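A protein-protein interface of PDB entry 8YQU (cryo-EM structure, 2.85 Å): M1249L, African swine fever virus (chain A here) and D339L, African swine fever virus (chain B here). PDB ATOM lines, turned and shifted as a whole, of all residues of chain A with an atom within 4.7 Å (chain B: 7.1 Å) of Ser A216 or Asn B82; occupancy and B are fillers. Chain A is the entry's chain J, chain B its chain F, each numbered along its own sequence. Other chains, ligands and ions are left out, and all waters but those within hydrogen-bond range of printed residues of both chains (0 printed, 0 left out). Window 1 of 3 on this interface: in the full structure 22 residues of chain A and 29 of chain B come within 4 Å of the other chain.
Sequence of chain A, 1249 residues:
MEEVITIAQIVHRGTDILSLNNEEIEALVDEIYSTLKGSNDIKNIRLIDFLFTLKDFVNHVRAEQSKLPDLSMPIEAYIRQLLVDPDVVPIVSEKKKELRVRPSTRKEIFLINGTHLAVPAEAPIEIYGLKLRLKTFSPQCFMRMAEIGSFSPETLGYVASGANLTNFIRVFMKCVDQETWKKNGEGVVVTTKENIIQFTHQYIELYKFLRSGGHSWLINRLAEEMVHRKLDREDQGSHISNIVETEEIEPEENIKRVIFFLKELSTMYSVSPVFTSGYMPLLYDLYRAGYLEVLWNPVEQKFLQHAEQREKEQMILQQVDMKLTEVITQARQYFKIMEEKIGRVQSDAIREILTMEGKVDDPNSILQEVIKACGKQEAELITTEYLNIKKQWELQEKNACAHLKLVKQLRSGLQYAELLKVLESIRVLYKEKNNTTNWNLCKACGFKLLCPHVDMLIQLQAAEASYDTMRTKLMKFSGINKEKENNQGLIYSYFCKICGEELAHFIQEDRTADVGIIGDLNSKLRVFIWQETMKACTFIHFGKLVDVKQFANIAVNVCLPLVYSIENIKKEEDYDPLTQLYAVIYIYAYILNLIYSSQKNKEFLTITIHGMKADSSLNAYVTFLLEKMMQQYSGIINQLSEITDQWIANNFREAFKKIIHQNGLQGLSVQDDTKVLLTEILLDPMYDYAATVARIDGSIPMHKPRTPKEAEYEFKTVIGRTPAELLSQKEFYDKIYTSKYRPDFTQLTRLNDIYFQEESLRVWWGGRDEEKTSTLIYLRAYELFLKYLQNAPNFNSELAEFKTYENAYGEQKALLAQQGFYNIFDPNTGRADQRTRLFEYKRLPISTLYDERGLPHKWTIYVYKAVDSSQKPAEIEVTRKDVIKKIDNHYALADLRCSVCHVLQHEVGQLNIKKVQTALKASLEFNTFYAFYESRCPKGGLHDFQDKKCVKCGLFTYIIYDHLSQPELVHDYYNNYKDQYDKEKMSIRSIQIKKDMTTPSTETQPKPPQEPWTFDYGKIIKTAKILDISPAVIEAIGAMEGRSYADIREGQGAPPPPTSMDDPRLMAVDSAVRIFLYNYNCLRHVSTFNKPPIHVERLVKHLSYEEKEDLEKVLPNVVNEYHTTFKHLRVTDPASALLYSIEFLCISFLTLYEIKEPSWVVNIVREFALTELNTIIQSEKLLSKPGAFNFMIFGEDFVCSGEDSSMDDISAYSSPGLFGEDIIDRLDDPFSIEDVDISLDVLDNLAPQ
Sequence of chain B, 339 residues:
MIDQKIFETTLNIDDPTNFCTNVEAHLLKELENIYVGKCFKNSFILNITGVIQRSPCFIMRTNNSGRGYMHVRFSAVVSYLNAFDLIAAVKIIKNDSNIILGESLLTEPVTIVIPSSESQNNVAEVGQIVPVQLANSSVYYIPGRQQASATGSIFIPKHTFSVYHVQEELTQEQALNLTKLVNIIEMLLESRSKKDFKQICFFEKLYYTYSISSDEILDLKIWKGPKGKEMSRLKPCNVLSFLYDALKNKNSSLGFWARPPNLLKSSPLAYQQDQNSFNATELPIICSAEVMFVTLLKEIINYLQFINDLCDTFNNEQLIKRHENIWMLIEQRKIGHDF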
ATOM      1  N   PRO A 153      22.252 -22.134  -5.639  1.00  0.00           N
ATOM      2  CA  PRO A 153      22.366 -21.791  -4.212  1.00  0.00           C
ATOM      3  C   PRO A 153      22.962 -22.898  -3.362  1.00  0.00           C
ATOM      4  O   PRO A 153      23.597 -22.602  -2.343  1.00  0.00           O
ATOM      5  CB  PRO A 153      20.915 -21.489  -3.812  1.00  0.00           C
ATOM      6  CG  PRO A 153      20.265 -21.056  -5.081  1.00  0.00           C
ATOM      7  CD  PRO A 153      20.894 -21.896  -6.156  1.00  0.00           C
ATOM      8  N   SER A 212      16.098 -26.070  -0.429  1.00  0.00           N
ATOM      9  CA  SER A 212      14.742 -25.572  -0.265  1.00  0.00           C
ATOM     10  C   SER A 212      14.663 -24.080  -0.581  1.00  0.00           C
ATOM     11  O   SER A 212      15.639 -23.446  -0.992  1.00  0.00           O
ATOM     12  CB  SER A 212      14.245 -25.852   1.151  1.00  0.00           C
ATOM     13  OG  SER A 212      14.189 -27.245   1.407  1.00  0.00           O
ATOM     14  N   GLY A 213      13.467 -23.514  -0.394  1.00  0.00           N
ATOM     15  CA  GLY A 213      13.289 -22.086  -0.605  1.00  0.00           C
ATOM     16  C   GLY A 213      14.133 -21.254   0.340  1.00  0.00           C
ATOM     17  O   GLY A 213      14.698 -20.231  -0.054  1.00  0.00           O
ATOM     18  N   GLY A 214      14.223 -21.677   1.597  1.00  0.00           N
ATOM     19  CA  GLY A 214      15.178 -21.074   2.502  1.00  0.00           C
ATOM     20  C   GLY A 214      16.601 -21.381   2.078  1.00  0.00           C
ATOM     21  O   GLY A 214      16.856 -22.296   1.293  1.00  0.00           O
ATOM     22  N   HIS A 215      17.533 -20.562   2.572  1.00  0.00           N
ATOM     23  CA  HIS A 215      18.960 -20.674   2.275  1.00  0.00           C
ATOM     24  C   HIS A 215      19.247 -20.249   0.838  1.00  0.00           C
ATOM     25  O   HIS A 215      20.407 -20.088   0.449  1.00  0.00           O
ATOM     26  CB  HIS A 215      19.462 -22.101   2.531  1.00  0.00           C
ATOM     27  CG  HIS A 215      20.907 -22.306   2.205  1.00  0.00           C
ATOM     28  ND1 HIS A 215      21.923 -21.940   3.062  1.00  0.00           N
ATOM     29  CD2 HIS A 215      21.508 -22.825   1.109  1.00  0.00           C
ATOM     30  CE1 HIS A 215      23.087 -22.238   2.513  1.00  0.00           C
ATOM     31  NE2 HIS A 215      22.863 -22.770   1.325  1.00  0.00           N
ATOM     32  N   SER A 216      18.199 -20.038   0.045  1.00  0.00           N
ATOM     33  CA  SER A 216      18.352 -19.501  -1.298  1.00  0.00           C
ATOM     34  C   SER A 216      18.201 -17.992  -1.340  1.00  0.00           C
ATOM     35  O   SER A 216      18.959 -17.321  -2.048  1.00  0.00           O
ATOM     36  CB  SER A 216      17.333 -20.137  -2.247  1.00  0.00           C
ATOM     37  OG  SER A 216      16.013 -19.757  -1.898  1.00  0.00           O
ATOM     38  N   TRP A 217      17.237 -17.446  -0.600  1.00  0.00           N
ATOM     39  CA  TRP A 217      17.186 -16.005  -0.394  1.00  0.00           C
ATOM     40  C   TRP A 217      18.415 -15.520   0.362  1.00  0.00           C
ATOM     41  O   TRP A 217      19.006 -14.491   0.015  1.00  0.00           O
ATOM     42  CB  TRP A 217      15.916 -15.628   0.368  1.00  0.00           C
ATOM     43  CG  TRP A 217      15.977 -14.254   0.954  1.00  0.00           C
ATOM     44  CD1 TRP A 217      15.805 -13.074   0.296  1.00  0.00           C
ATOM     45  CD2 TRP A 217      16.273 -13.916   2.314  1.00  0.00           C
ATOM     46  NE1 TRP A 217      15.952 -12.020   1.166  1.00  0.00           N
ATOM     47  CE2 TRP A 217      16.242 -12.512   2.411  1.00  0.00           C
ATOM     48  CE3 TRP A 217      16.552 -14.666   3.461  1.00  0.00           C
ATOM     49  CZ2 TRP A 217      16.480 -11.841   3.609  1.00  0.00           C
ATOM     50  CZ3 TRP A 217      16.789 -13.999   4.648  1.00  0.00           C
ATOM     51  CH2 TRP A 217      16.751 -12.601   4.713  1.00  0.00           C
ATOM     52  N   LEU A 218      18.818 -16.258   1.399  1.00  0.00           N
ATOM     53  CA  LEU A 218      19.864 -15.783   2.299  1.00  0.00           C
ATOM     54  C   LEU A 218      21.224 -15.746   1.611  1.00  0.00           C
ATOM     55  O   LEU A 218      21.934 -14.733   1.674  1.00  0.00           O
ATOM     56  CB  LEU A 218      19.901 -16.666   3.549  1.00  0.00           C
ATOM     57  CG  LEU A 218      20.765 -16.235   4.736  1.00  0.00           C
ATOM     58  CD1 LEU A 218      20.032 -16.499   6.039  1.00  0.00           C
ATOM     59  CD2 LEU A 218      22.081 -16.986   4.725  1.00  0.00           C
ATOM     60  N   ILE A 219      21.604 -16.835   0.940  1.00  0.00           N
ATOM     61  CA  ILE A 219      22.934 -16.908   0.340  1.00  0.00           C
ATOM     62  C   ILE A 219      23.046 -15.963  -0.849  1.00  0.00           C
ATOM     63  O   ILE A 219      24.056 -15.270  -1.013  1.00  0.00           O
ATOM     64  CB  ILE A 219      23.275 -18.354  -0.053  1.00  0.00           C
ATOM     65  CG1 ILE A 219      23.261 -19.247   1.184  1.00  0.00           C
ATOM     66  CG2 ILE A 219      24.631 -18.416  -0.729  1.00  0.00           C
ATOM     67  CD1 ILE A 219      24.271 -18.849   2.234  1.00  0.00           C
ATOM     68  N   ASN A 220      22.020 -15.926  -1.702  1.00  0.00           N
ATOM     69  CA  ASN A 220      22.052 -15.004  -2.832  1.00  0.00           C
ATOM     70  C   ASN A 220      22.125 -13.559  -2.354  1.00  0.00           C
ATOM     71  O   ASN A 220      22.899 -12.755  -2.891  1.00  0.00           O
ATOM     72  CB  ASN A 220      20.829 -15.217  -3.724  1.00  0.00           C
ATOM     73  CG  ASN A 220      20.985 -16.405  -4.654  1.00  0.00           C
ATOM     74  OD1 ASN A 220      20.250 -17.387  -4.556  1.00  0.00           O
ATOM     75  ND2 ASN A 220      21.949 -16.321  -5.564  1.00  0.00           N
ATOM     76  N   MET B   1      11.221 -15.597  -5.954  1.00  0.00           N
ATOM     77  CA  MET B   1      11.129 -14.279  -5.339  1.00  0.00           C
ATOM     78  C   MET B   1      11.460 -13.181  -6.341  1.00  0.00           C
ATOM     79  O   MET B   1      11.652 -13.447  -7.524  1.00  0.00           O
ATOM     80  CB  MET B   1      12.067 -14.181  -4.135  1.00  0.00           C
ATOM     81  CG  MET B   1      11.688 -15.079  -2.970  1.00  0.00           C
ATOM     82  SD  MET B   1      12.871 -14.974  -1.613  1.00  0.00           S
ATOM     83  CE  MET B   1      12.533 -13.327  -0.997  1.00  0.00           C
ATOM     84  N   ASP B   3      14.275 -10.161  -6.337  1.00  0.00           N
ATOM     85  CA  ASP B   3      15.406  -9.723  -5.532  1.00  0.00           C
ATOM     86  C   ASP B   3      16.486  -9.142  -6.436  1.00  0.00           C
ATOM     87  O   ASP B   3      16.495  -9.348  -7.652  1.00  0.00           O
ATOM     88  CB  ASP B   3      15.949 -10.882  -4.683  1.00  0.00           C
ATOM     89  CG  ASP B   3      16.956 -10.430  -3.640  1.00  0.00           C
ATOM     90  OD1 ASP B   3      17.263  -9.220  -3.584  1.00  0.00           O
ATOM     91  OD2 ASP B   3      17.437 -11.288  -2.871  1.00  0.00           O
ATOM     92  N   TYR B  80      14.237 -15.387  -8.902  1.00  0.00           N
ATOM     93  CA  TYR B  80      14.657 -16.774  -8.749  1.00  0.00           C
ATOM     94  C   TYR B  80      13.520 -17.546  -8.095  1.00  0.00           C
ATOM     95  O   TYR B  80      13.091 -17.205  -6.987  1.00  0.00           O
ATOM     96  CB  TYR B  80      15.934 -16.883  -7.916  1.00  0.00           C
ATOM     97  CG  TYR B  80      16.608 -18.234  -8.020  1.00  0.00           C
ATOM     98  CD1 TYR B  80      16.161 -19.317  -7.274  1.00  0.00           C
ATOM     99  CD2 TYR B  80      17.684 -18.429  -8.874  1.00  0.00           C
ATOM    100  CE1 TYR B  80      16.771 -20.553  -7.371  1.00  0.00           C
ATOM    101  CE2 TYR B  80      18.300 -19.662  -8.978  1.00  0.00           C
ATOM    102  CZ  TYR B  80      17.839 -20.721  -8.225  1.00  0.00           C
ATOM    103  OH  TYR B  80      18.451 -21.949  -8.327  1.00  0.00           O
ATOM    104  N   LEU B  81      13.039 -18.580  -8.776  1.00  0.00           N
ATOM    105  CA  LEU B  81      11.950 -19.398  -8.264  1.00  0.00           C
ATOM    106  C   LEU B  81      12.520 -20.664  -7.639  1.00  0.00           C
ATOM    107  O   LEU B  81      13.314 -21.372  -8.266  1.00  0.00           O
ATOM    108  CB  LEU B  81      10.964 -19.749  -9.377  1.00  0.00           C
ATOM    109  CG  LEU B  81       9.553 -20.091  -8.898  1.00  0.00           C
ATOM    110  CD1 LEU B  81       8.955 -18.920  -8.135  1.00  0.00           C
ATOM    111  CD2 LEU B  81       8.668 -20.480 -10.065  1.00  0.00           C
ATOM    112  N   ASN B  82      12.117 -20.940  -6.404  1.00  0.00           N
ATOM    113  CA  ASN B  82      12.646 -22.067  -5.655  1.00  0.00           C
ATOM    114  C   ASN B  82      11.737 -23.281  -5.832  1.00  0.00           C
ATOM    115  O   ASN B  82      10.804 -23.280  -6.640  1.00  0.00           O
ATOM    116  CB  ASN B  82      12.805 -21.688  -4.186  1.00  0.00           C
ATOM    117  CG  ASN B  82      13.804 -20.573  -3.981  1.00  0.00           C
ATOM    118  OD1 ASN B  82      14.993 -20.734  -4.256  1.00  0.00           O
ATOM    119  ND2 ASN B  82      13.328 -19.430  -3.501  1.00  0.00           N
ATOM    120  N   ALA B  83      12.005 -24.335  -5.070  1.00  0.00           N
ATOM    121  CA  ALA B  83      11.169 -25.523  -5.047  1.00  0.00           C
ATOM    122  C   ALA B  83      10.109 -25.391  -3.962  1.00  0.00           C
ATOM    123  O   ALA B  83      10.253 -24.619  -3.011  1.00  0.00           O
ATOM    124  CB  ALA B  83      12.012 -26.780  -4.811  1.00  0.00           C
ATOM    125  N   PHE B  84       9.034 -26.165  -4.120  1.00  0.00           N
ATOM    126  CA  PHE B  84       7.899 -26.145  -3.196  1.00  0.00           C
ATOM    127  C   PHE B  84       7.327 -24.736  -3.047  1.00  0.00           C
ATOM    128  O   PHE B  84       6.977 -24.300  -1.949  1.00  0.00           O
ATOM    129  CB  PHE B  84       8.283 -26.722  -1.831  1.00  0.00           C
ATOM    130  CG  PHE B  84       8.363 -28.221  -1.808  1.00  0.00           C
ATOM    131  CD1 PHE B  84       7.337 -28.991  -2.331  1.00  0.00           C
ATOM    132  CD2 PHE B  84       9.464 -28.861  -1.265  1.00  0.00           C
ATOM    133  CE1 PHE B  84       7.407 -30.371  -2.311  1.00  0.00           C
ATOM    134  CE2 PHE B  84       9.541 -30.240  -1.242  1.00  0.00           C
ATOM    135  CZ  PHE B  84       8.511 -30.996  -1.766  1.00  0.00           C
ATOM    136  N   ASP B  85       7.231 -24.019  -4.161  1.00  0.00           N
ATOM    137  CA  ASP B  85       6.710 -22.661  -4.178  1.00  0.00           C
ATOM    138  C   ASP B  85       5.299 -22.643  -4.755  1.00  0.00           C
ATOM    139  O   ASP B  85       4.928 -23.476  -5.586  1.00  0.00           O
ATOM    140  CB  ASP B  85       7.625 -21.738  -4.987  1.00  0.00           C
ATOM    141  CG  ASP B  85       7.214 -20.281  -4.895  1.00  0.00           C
ATOM    142  OD1 ASP B  85       7.451 -19.662  -3.836  1.00  0.00           O
ATOM    143  OD2 ASP B  85       6.653 -19.755  -5.879  1.00  0.00           O
ATOM    144  N   LEU B  86       4.510 -21.674  -4.300  1.00  0.00           N
ATOM    145  CA  LEU B  86       3.107 -21.560  -4.674  1.00  0.00           C
ATOM    146  C   LEU B  86       2.934 -20.525  -5.776  1.00  0.00           C
ATOM    147  O   LEU B  86       3.377 -19.379  -5.639  1.00  0.00           O
ATOM    148  CB  LEU B  86       2.252 -21.182  -3.464  1.00  0.00           C
ATOM    149  CG  LEU B  86       2.177 -22.214  -2.339  1.00  0.00           C
ATOM    150  CD1 LEU B  86       1.933 -21.546  -0.997  1.00  0.00           C
ATOM    151  CD2 LEU B  86       1.076 -23.205  -2.642  1.00  0.00           C
ATOM    152  N   LEU B 134       4.959 -26.545  -6.741  1.00  0.00           N
ATOM    153  CA  LEU B 134       6.205 -26.950  -7.372  1.00  0.00           C
ATOM    154  C   LEU B 134       6.805 -28.150  -6.650  1.00  0.00           C
ATOM    155  O   LEU B 134       6.737 -28.262  -5.422  1.00  0.00           O
ATOM    156  CB  LEU B 134       7.210 -25.796  -7.386  1.00  0.00           C
ATOM    157  CG  LEU B 134       6.849 -24.565  -8.220  1.00  0.00           C
ATOM    158  CD1 LEU B 134       8.106 -23.807  -8.608  1.00  0.00           C
ATOM    159  CD2 LEU B 134       6.063 -24.959  -9.460  1.00  0.00           C
ATOM    160  N   ALA B 135       7.394 -29.052  -7.430  1.00  0.00           N
ATOM    161  CA  ALA B 135       8.003 -30.254  -6.886  1.00  0.00           C
ATOM    162  C   ALA B 135       9.363 -29.927  -6.273  1.00  0.00           C
ATOM    163  O   ALA B 135       9.859 -28.799  -6.351  1.00  0.00           O
ATOM    164  CB  ALA B 135       8.129 -31.323  -7.968  1.00  0.00           C
ATOM    165  N   SER B 137      12.375 -30.030  -7.037  1.00  0.00           N
ATOM    166  CA  SER B 137      13.358 -30.019  -8.108  1.00  0.00           C
ATOM    167  C   SER B 137      13.714 -28.578  -8.444  1.00  0.00           C
ATOM    168  O   SER B 137      12.895 -27.669  -8.295  1.00  0.00           O
ATOM    169  CB  SER B 137      12.844 -30.740  -9.362  1.00  0.00           C
ATOM    170  OG  SER B 137      12.626 -32.116  -9.105  1.00  0.00           O
ATOM    171  N   SER B 138      14.948 -28.383  -8.899  1.00  0.00           N
ATOM    172  CA  SER B 138      15.415 -27.048  -9.246  1.00  0.00           C
ATOM    173  C   SER B 138      14.697 -26.532 -10.487  1.00  0.00           C
ATOM    174  O   SER B 138      14.411 -27.287 -11.420  1.00  0.00           O
ATOM    175  CB  SER B 138      16.925 -27.057  -9.479  1.00  0.00           C
ATOM    176  OG  SER B 138      17.274 -27.964 -10.510  1.00  0.00           O
ATOM    177  N   VAL B 139      14.405 -25.235 -10.491  1.00  0.00           N
ATOM    178  CA  VAL B 139      13.759 -24.597 -11.633  1.00  0.00           C
ATOM    179  C   VAL B 139      14.811 -24.342 -12.704  1.00  0.00           C
ATOM    180  O   VAL B 139      15.836 -23.702 -12.443  1.00  0.00           O
ATOM    181  CB  VAL B 139      13.064 -23.293 -11.217  1.00  0.00           C
ATOM    182  CG1 VAL B 139      12.492 -22.587 -12.434  1.00  0.00           C
ATOM    183  CG2 VAL B 139      11.969 -23.583 -10.205  1.00  0.00           C
ATOM    184  N   TYR B 141      16.646 -22.732 -15.813  1.00  0.00           N
ATOM    185  CA  TYR B 141      16.810 -21.354 -16.263  1.00  0.00           C
ATOM    186  C   TYR B 141      17.670 -21.305 -17.517  1.00  0.00           C
ATOM    187  O   TYR B 141      18.668 -20.584 -17.588  1.00  0.00           O
ATOM    188  CB  TYR B 141      17.403 -20.487 -15.157  1.00  0.00           C
ATOM    189  CG  TYR B 141      16.394 -20.058 -14.117  1.00  0.00           C
ATOM    190  CD1 TYR B 141      15.378 -19.168 -14.437  1.00  0.00           C
ATOM    191  CD2 TYR B 141      16.455 -20.545 -12.819  1.00  0.00           C
ATOM    192  CE1 TYR B 141      14.453 -18.773 -13.491  1.00  0.00           C
ATOM    193  CE2 TYR B 141      15.532 -20.156 -11.867  1.00  0.00           C
ATOM    194  CZ  TYR B 141      14.534 -19.270 -12.208  1.00  0.00           C
ATOM    195  OH  TYR B 141      13.613 -18.879 -11.265  1.00  0.00           O
ATOM    196  N   ALA B 150      10.024 -25.396 -15.254  1.00  0.00           N
ATOM    197  CA  ALA B 150       9.930 -26.016 -13.943  1.00  0.00           C
ATOM    198  C   ALA B 150       8.758 -26.984 -13.922  1.00  0.00           C
ATOM    199  O   ALA B 150       7.708 -26.711 -14.509  1.00  0.00           O
ATOM    200  CB  ALA B 150       9.763 -24.969 -12.838  1.00  0.00           C
ATOM    201  N   VAL B 294      14.432 -19.074   9.037  1.00  0.00           N
ATOM    202  CA  VAL B 294      14.363 -18.741   7.621  1.00  0.00           C
ATOM    203  C   VAL B 294      13.327 -19.612   6.917  1.00  0.00           C
ATOM    204  O   VAL B 294      12.570 -19.125   6.072  1.00  0.00           O
ATOM    205  CB  VAL B 294      15.755 -18.828   6.965  1.00  0.00           C
ATOM    206  CG1 VAL B 294      16.211 -20.263   6.795  1.00  0.00           C
ATOM    207  CG2 VAL B 294      15.754 -18.106   5.626  1.00  0.00           C
ATOM    208  N   LYS B 298       9.996 -18.089   5.300  1.00  0.00           N
ATOM    209  CA  LYS B 298       9.802 -18.332   3.875  1.00  0.00           C
ATOM    210  C   LYS B 298       8.457 -18.993   3.610  1.00  0.00           C
ATOM    211  O   LYS B 298       7.785 -18.674   2.623  1.00  0.00           O
ATOM    212  CB  LYS B 298      10.942 -19.190   3.329  1.00  0.00           C
ATOM    213  CG  LYS B 298      10.866 -19.443   1.835  1.00  0.00           C
ATOM    214  CD  LYS B 298      11.085 -18.160   1.052  1.00  0.00           C
ATOM    215  CE  LYS B 298      11.177 -18.434  -0.440  1.00  0.00           C
ATOM    216  NZ  LYS B 298       9.915 -19.014  -0.974  1.00  0.00           N
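Among the printed residues, pairs that only touch across the chains: Pro A153 with Tyr B80 (3.3 Å), Gly A213 with Asn B82 (3.6 Å), Gly A213 with Lys B298 (3.97 Å), Trp A217 with Met B1 (3.5 Å) and Trp A217 with Asp B3 (3.99 Å).
The side-chain amide oxygen (OD1) of Asn B82 lies within hydrogen-bond range of the side-chain hydroxyl (OG) of Ser A216 (2.7 Å).
Printed residues of chain B within 4 Å of Pro A153: Tyr B80 (3.3 Å). Of the printed residues of chain B, Gly A213 touches Asn B82 and Lys B298. Of chain B, only Asn B82 (2.7 Å) comes within 4 Å of Ser A216. Printed residues of chain B within 4 Å of Trp A217: Met B1 (3.5 Å) and Asp B3 (3.99 Å). Of the printed residues of chain A, Asp B3 touches Trp A217 (3.99 Å). Printed residues of chain A within 4 Å of Tyr B80: Pro A153. Asn B82 touches just these residues of chain A: Gly A213 (3.6 Å) and Ser A216 (2.7 Å). The nearest residue of chain A that does not touch Asn B82 is Ser A212 (4.3 Å). The nearest printed residue of chain B that does not touch Pro A153 is Asn B82 (5.3 Å).
Hydrophobic or aromatic side chains of chain A that line the printed part of chain B: Pro A153 and Trp A217. Hydrophobic or aromatic side chains of chain B that line the printed part of chain A: Met B1 and Tyr B80. Along chain B the printed residues that touch a printed residue of chain A span positions 1 to 298. Among the printed residues, no Asp or Glu carboxylate lies within 4 Å of a Lys or Arg side-chain nitrogen of the other chain.
The backbone NH (N) of Met B1 lies within hydrogen-bond range of the backbone carbonyl oxygen (O) of Tyr B80, at 2.7 Å. O of Ser A216 lies close to OD1 of Asn A220. NZ of Lys B298 is in salt-bridge range of OD1 of Asp B85 (3.8 Å).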
